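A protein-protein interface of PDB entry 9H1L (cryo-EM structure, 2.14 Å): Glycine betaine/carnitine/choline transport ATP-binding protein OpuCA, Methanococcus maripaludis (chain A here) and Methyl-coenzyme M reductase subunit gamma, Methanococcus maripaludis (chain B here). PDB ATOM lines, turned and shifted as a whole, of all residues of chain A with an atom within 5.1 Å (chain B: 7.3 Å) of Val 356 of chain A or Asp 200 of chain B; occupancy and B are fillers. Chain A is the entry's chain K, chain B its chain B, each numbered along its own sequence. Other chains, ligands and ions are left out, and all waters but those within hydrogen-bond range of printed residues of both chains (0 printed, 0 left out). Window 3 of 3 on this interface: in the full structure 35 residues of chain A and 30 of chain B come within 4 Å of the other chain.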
ATOM      1  N   ALA A 333      13.011  26.205 -11.297  1.00  0.00           N
ATOM      2  CA  ALA A 333      11.677  26.091 -11.900  1.00  0.00           C
ATOM      3  C   ALA A 333      10.683  27.057 -11.261  1.00  0.00           C
ATOM      4  O   ALA A 333       9.509  26.737 -11.070  1.00  0.00           O
ATOM      5  CB  ALA A 333      11.158  24.651 -11.856  1.00  0.00           C
ATOM      6  N   THR A 354      10.514  23.027 -18.970  1.00  0.00           N
ATOM      7  CA  THR A 354       9.799  24.317 -19.153  1.00  0.00           C
ATOM      8  C   THR A 354       8.376  23.801 -19.403  1.00  0.00           C
ATOM      9  O   THR A 354       7.720  24.352 -20.299  1.00  0.00           O
ATOM     10  CB  THR A 354      10.608  24.381 -20.458  1.00  0.00           C
ATOM     11  OG1 THR A 354      10.307  23.227 -21.242  1.00  0.00           O
ATOM     12  CG2 THR A 354      12.102  24.466 -20.228  1.00  0.00           C
ATOM     13  N   LYS A 355       7.919  22.789 -18.660  1.00  0.00           N
ATOM     14  CA  LYS A 355       6.531  22.274 -18.761  1.00  0.00           C
ATOM     15  C   LYS A 355       6.001  22.163 -17.333  1.00  0.00           C
ATOM     16  O   LYS A 355       6.554  21.356 -16.575  1.00  0.00           O
ATOM     17  CB  LYS A 355       6.492  20.903 -19.431  1.00  0.00           C
ATOM     18  CG  LYS A 355       6.837  20.889 -20.913  1.00  0.00           C
ATOM     19  CD  LYS A 355       7.739  19.740 -21.295  1.00  0.00           C
ATOM     20  CE  LYS A 355       7.154  18.391 -20.936  1.00  0.00           C
ATOM     21  NZ  LYS A 355       7.980  17.681 -19.933  1.00  0.00           N
ATOM     22  N   VAL A 356       4.987  22.949 -16.987  1.00  0.00           N
ATOM     23  CA  VAL A 356       4.482  22.972 -15.588  1.00  0.00           C
ATOM     24  C   VAL A 356       3.680  21.702 -15.294  1.00  0.00           C
ATOM     25  O   VAL A 356       3.111  21.135 -16.233  1.00  0.00           O
ATOM     26  CB  VAL A 356       3.634  24.231 -15.350  1.00  0.00           C
ATOM     27  CG1 VAL A 356       4.487  25.491 -15.389  1.00  0.00           C
ATOM     28  CG2 VAL A 356       2.491  24.335 -16.344  1.00  0.00           C
ATOM     29  N   GLY A 357       3.639  21.280 -14.031  1.00  0.00           N
ATOM     30  CA  GLY A 357       2.801  20.127 -13.662  1.00  0.00           C
ATOM     31  C   GLY A 357       3.566  19.048 -12.931  1.00  0.00           C
ATOM     32  O   GLY A 357       4.794  18.997 -13.072  1.00  0.00           O
ATOM     33  N   PRO A 358       2.884  18.174 -12.165  1.00  0.00           N
ATOM     34  CA  PRO A 358       3.550  17.061 -11.496  1.00  0.00           C
ATOM     35  C   PRO A 358       4.112  16.054 -12.506  1.00  0.00           C
ATOM     36  O   PRO A 358       5.136  15.486 -12.227  1.00  0.00           O
ATOM     37  CB  PRO A 358       2.411  16.425 -10.693  1.00  0.00           C
ATOM     38  CG  PRO A 358       1.366  17.505 -10.574  1.00  0.00           C
ATOM     39  CD  PRO A 358       1.453  18.242 -11.889  1.00  0.00           C
ATOM     40  N   TYR A 360       5.520  16.694 -15.119  1.00  0.00           N
ATOM     41  CA  TYR A 360       6.748  17.265 -15.734  1.00  0.00           C
ATOM     42  C   TYR A 360       7.887  18.087 -15.122  1.00  0.00           C
ATOM     43  O   TYR A 360       9.050  17.704 -15.316  1.00  0.00           O
ATOM     44  CB  TYR A 360       6.374  18.189 -16.894  1.00  0.00           C
ATOM     45  CG  TYR A 360       5.122  17.778 -17.625  1.00  0.00           C
ATOM     46  CD1 TYR A 360       5.127  16.711 -18.508  1.00  0.00           C
ATOM     47  CD2 TYR A 360       3.925  18.436 -17.413  1.00  0.00           C
ATOM     48  CE1 TYR A 360       3.979  16.320 -19.173  1.00  0.00           C
ATOM     49  CE2 TYR A 360       2.767  18.060 -18.069  1.00  0.00           C
ATOM     50  CZ  TYR A 360       2.794  16.997 -18.954  1.00  0.00           C
ATOM     51  OH  TYR A 360       1.650  16.616 -19.610  1.00  0.00           O
ATOM     52  N   ARG A 361       7.565  19.173 -14.411  1.00  0.00           N
ATOM     53  CA  ARG A 361       8.607  20.072 -13.839  1.00  0.00           C
ATOM     54  C   ARG A 361       8.503  19.495 -12.423  1.00  0.00           C
ATOM     55  O   ARG A 361       9.559  19.158 -11.852  1.00  0.00           O
ATOM     56  CB  ARG A 361       8.207  21.549 -13.827  1.00  0.00           C
ATOM     57  CG  ARG A 361       9.186  22.459 -14.553  1.00  0.00           C
ATOM     58  CD  ARG A 361       8.512  23.704 -15.093  1.00  0.00           C
ATOM     59  NE  ARG A 361       7.660  24.330 -14.093  1.00  0.00           N
ATOM     60  CZ  ARG A 361       7.827  25.565 -13.637  1.00  0.00           C
ATOM     61  NH1 ARG A 361       8.606  26.411 -14.288  1.00  0.00           N
ATOM     62  NH2 ARG A 361       7.215  25.952 -12.532  1.00  0.00           N
ATOM     63  N   GLY A 362       7.286  19.404 -11.878  1.00  0.00           N
ATOM     64  CA  GLY A 362       7.088  18.898 -10.505  1.00  0.00           C
ATOM     65  C   GLY A 362       8.026  17.755 -10.164  1.00  0.00           C
ATOM     66  O   GLY A 362       8.636  17.802  -9.081  1.00  0.00           O
ATOM     67  N   LYS A 365      11.071  19.127  -9.091  1.00  0.00           N
ATOM     68  CA  LYS A 365      10.915  20.215  -8.134  1.00  0.00           C
ATOM     69  C   LYS A 365      10.743  19.732  -6.704  1.00  0.00           C
ATOM     70  O   LYS A 365      10.830  20.550  -5.784  1.00  0.00           O
ATOM     71  CB  LYS A 365       9.732  21.090  -8.531  1.00  0.00           C
ATOM     72  CG  LYS A 365      10.134  22.451  -9.050  1.00  0.00           C
ATOM     73  CD  LYS A 365       8.936  23.360  -9.182  1.00  0.00           C
ATOM     74  CE  LYS A 365       8.760  24.232  -7.954  1.00  0.00           C
ATOM     75  NZ  LYS A 365       8.464  25.640  -8.325  1.00  0.00           N
ATOM     76  N   LYS B  41       1.245  28.649  -1.473  1.00  0.00           N
ATOM     77  CA  LYS B  41       1.226  28.122  -2.836  1.00  0.00           C
ATOM     78  C   LYS B  41      -0.185  28.085  -3.414  1.00  0.00           C
ATOM     79  O   LYS B  41      -0.382  28.399  -4.593  1.00  0.00           O
ATOM     80  CB  LYS B  41       1.850  26.729  -2.865  1.00  0.00           C
ATOM     81  CG  LYS B  41       3.314  26.717  -3.275  1.00  0.00           C
ATOM     82  CD  LYS B  41       4.054  25.498  -2.737  1.00  0.00           C
ATOM     83  CE  LYS B  41       3.237  24.221  -2.868  1.00  0.00           C
ATOM     84  NZ  LYS B  41       3.714  23.159  -1.939  1.00  0.00           N
ATOM     85  N   GLN B  47       5.969  33.598  -4.199  1.00  0.00           N
ATOM     86  CA  GLN B  47       6.743  32.375  -4.063  1.00  0.00           C
ATOM     87  C   GLN B  47       7.122  32.175  -2.600  1.00  0.00           C
ATOM     88  O   GLN B  47       7.587  33.121  -1.954  1.00  0.00           O
ATOM     89  CB  GLN B  47       7.993  32.447  -4.935  1.00  0.00           C
ATOM     90  CG  GLN B  47       8.960  31.297  -4.748  1.00  0.00           C
ATOM     91  CD  GLN B  47       8.422  29.992  -5.291  1.00  0.00           C
ATOM     92  OE1 GLN B  47       8.589  28.937  -4.680  1.00  0.00           O
ATOM     93  NE2 GLN B  47       7.777  30.055  -6.449  1.00  0.00           N
ATOM     94  N   VAL B 191      -4.740  20.929  -7.286  1.00  0.00           N
ATOM     95  CA  VAL B 191      -3.796  20.858  -8.397  1.00  0.00           C
ATOM     96  C   VAL B 191      -3.578  22.211  -9.056  1.00  0.00           C
ATOM     97  O   VAL B 191      -2.676  22.341  -9.899  1.00  0.00           O
ATOM     98  CB  VAL B 191      -4.261  19.834  -9.451  1.00  0.00           C
ATOM     99  CG1 VAL B 191      -4.343  18.449  -8.834  1.00  0.00           C
ATOM    100  CG2 VAL B 191      -5.602  20.242 -10.033  1.00  0.00           C
ATOM    101  N   LYS B 197      -3.802  28.867 -12.491  1.00  0.00           N
ATOM    102  CA  LYS B 197      -2.612  28.273 -13.081  1.00  0.00           C
ATOM    103  C   LYS B 197      -2.233  27.002 -12.324  1.00  0.00           C
ATOM    104  O   LYS B 197      -2.390  26.938 -11.103  1.00  0.00           O
ATOM    105  CB  LYS B 197      -1.432  29.249 -13.100  1.00  0.00           C
ATOM    106  CG  LYS B 197      -1.178  30.014 -11.824  1.00  0.00           C
ATOM    107  CD  LYS B 197      -0.606  31.388 -12.144  1.00  0.00           C
ATOM    108  CE  LYS B 197      -1.661  32.469 -12.102  1.00  0.00           C
ATOM    109  NZ  LYS B 197      -1.089  33.802 -11.766  1.00  0.00           N
ATOM    110  N   PRO B 198      -1.756  25.970 -13.022  1.00  0.00           N
ATOM    111  CA  PRO B 198      -1.485  24.690 -12.360  1.00  0.00           C
ATOM    112  C   PRO B 198      -0.315  24.769 -11.394  1.00  0.00           C
ATOM    113  O   PRO B 198       0.614  25.561 -11.560  1.00  0.00           O
ATOM    114  CB  PRO B 198      -1.172  23.741 -13.526  1.00  0.00           C
ATOM    115  CG  PRO B 198      -1.653  24.436 -14.753  1.00  0.00           C
ATOM    116  CD  PRO B 198      -1.548  25.895 -14.479  1.00  0.00           C
ATOM    117  N   LEU B 199      -0.381  23.925 -10.368  1.00  0.00           N
ATOM    118  CA  LEU B 199       0.682  23.813  -9.385  1.00  0.00           C
ATOM    119  C   LEU B 199       1.641  22.703  -9.792  1.00  0.00           C
ATOM    120  O   LEU B 199       1.231  21.690 -10.363  1.00  0.00           O
ATOM    121  CB  LEU B 199       0.110  23.532  -7.998  1.00  0.00           C
ATOM    122  CG  LEU B 199      -0.816  24.605  -7.429  1.00  0.00           C
ATOM    123  CD1 LEU B 199      -1.362  24.176  -6.084  1.00  0.00           C
ATOM    124  CD2 LEU B 199      -0.083  25.928  -7.316  1.00  0.00           C
ATOM    125  N   ASP B 200       2.926  22.910  -9.497  1.00  0.00           N
ATOM    126  CA  ASP B 200       3.935  21.919  -9.855  1.00  0.00           C
ATOM    127  C   ASP B 200       3.811  20.671  -8.991  1.00  0.00           C
ATOM    128  O   ASP B 200       4.033  19.554  -9.469  1.00  0.00           O
ATOM    129  CB  ASP B 200       5.323  22.539  -9.736  1.00  0.00           C
ATOM    130  CG  ASP B 200       5.476  23.770 -10.607  1.00  0.00           C
ATOM    131  OD1 ASP B 200       4.680  23.926 -11.550  1.00  0.00           O
ATOM    132  OD2 ASP B 200       6.383  24.587 -10.351  1.00  0.00           O
ATOM    133  N   ALA B 201       3.450  20.838  -7.723  1.00  0.00           N
ATOM    134  CA  ALA B 201       3.206  19.725  -6.821  1.00  0.00           C
ATOM    135  C   ALA B 201       1.812  19.875  -6.226  1.00  0.00           C
ATOM    136  O   ALA B 201       1.509  20.930  -5.645  1.00  0.00           O
ATOM    137  CB  ALA B 201       4.258  19.668  -5.713  1.00  0.00           C
ATOM    138  N   PRO B 202       0.932  18.882  -6.365  1.00  0.00           N
ATOM    139  CA  PRO B 202      -0.388  18.978  -5.733  1.00  0.00           C
ATOM    140  C   PRO B 202      -0.279  18.959  -4.218  1.00  0.00           C
ATOM    141  O   PRO B 202       0.570  18.274  -3.644  1.00  0.00           O
ATOM    142  CB  PRO B 202      -1.126  17.743  -6.261  1.00  0.00           C
ATOM    143  CG  PRO B 202      -0.048  16.783  -6.615  1.00  0.00           C
ATOM    144  CD  PRO B 202       1.113  17.610  -7.082  1.00  0.00           C
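Hydrophobic or aromatic side chains of chain B within 4 Å of the printed part of chain A: Pro 202. Hydrophobic or aromatic side chains of chain A within 4 Å of the printed part of chain B: Val 356 and Pro 358.
Val 356 of chain A touches one residue of chain B. Asp 200 of chain B touches just these residues of chain A: Ala 333, Val 356, Gly 357, Pro 358, Arg 361, Gly 362 and Lys 365. Of the printed residues of chain B, Pro 358 of chain A touches Leu 199 (3.8 Å), Asp 200 (3.2 Å) and Pro 202 (3.5 Å). Printed residues of chain B within 4 Å of Lys 365 of chain A: Asp 200. Printed residues of chain B within 4 Å of Gly 362 of chain A: Asp 200. Printed residues of chain B within 4 Å of Arg 361 of chain A: Asp 200. Thr 354 of chain A touches none of the printed residues of chain B. Lys 41 of chain B touches none of the printed residues of chain A. The nearest residue of chain B that does not touch Val 356 of chain A is Pro 198 of chain B (4.4 Å). The nearest printed residue of chain A that does not touch Asp 200 of chain B is Lys 355 of chain A (5.9 Å). The nearest printed residue of chain A that does not touch Leu 199 of chain B is Val 356 of chain A (5.5 Å).
The guanidinium group (NH2) of Arg 361 of chain A lies within salt-bridge range of the side-chain carboxylate (OD2) of Asp 200 of chain B, 2.7 Å away. OD2 of Asp 200 of chain B is in salt-bridge range of NZ of Lys 365 of chain A, 3.1 Å away. The backbone nitrogen of Pro 358 of chain A sits close to the backbone carbonyl oxygen of Asp 200 of chain B.
O of Lys 355 of chain A lies close to N of Arg 361 of chain A, 3.2 Å away. The side-chain amino group (NZ) of Lys 365 of chain A is in hydrogen-bond range of the backbone carbonyl oxygen (O) of Ala 333 of chain A (3.1 Å). The backbone carbonyl oxygen (O) of Val 191 of chain B is in hydrogen-bond range of the backbone NH (N) of Leu 199 of chain B (2.8 Å). NH2 of Arg 361 of chain A lies within hydrogen-bond range of O of Ala 333 of chain A (2.8 Å). The backbone NH of Gly 362 of chain A is in hydrogen-bond range of the backbone carbonyl oxygen of Gly 357 of chain A.
Ala 333 of chain A touches Asp 200 of chain B. OD1 of Asp 200 of chain B touches CB of Val 356 of chain A, 3.95 Å away. Leu 199 of chain B touches Gly 357 of chain A (O to CA, 3.97 Å). Asp 200 of chain B touches Gly 357 of chain A. Leu 199 of chain B touches Pro 358 of chain A (O to CD, 3.8 Å). Pro 358 of chain A touches Pro 202 of chain B. CA of Gly 362 of chain A touches O of Asp 200 of chain B, 3.3 Å away.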
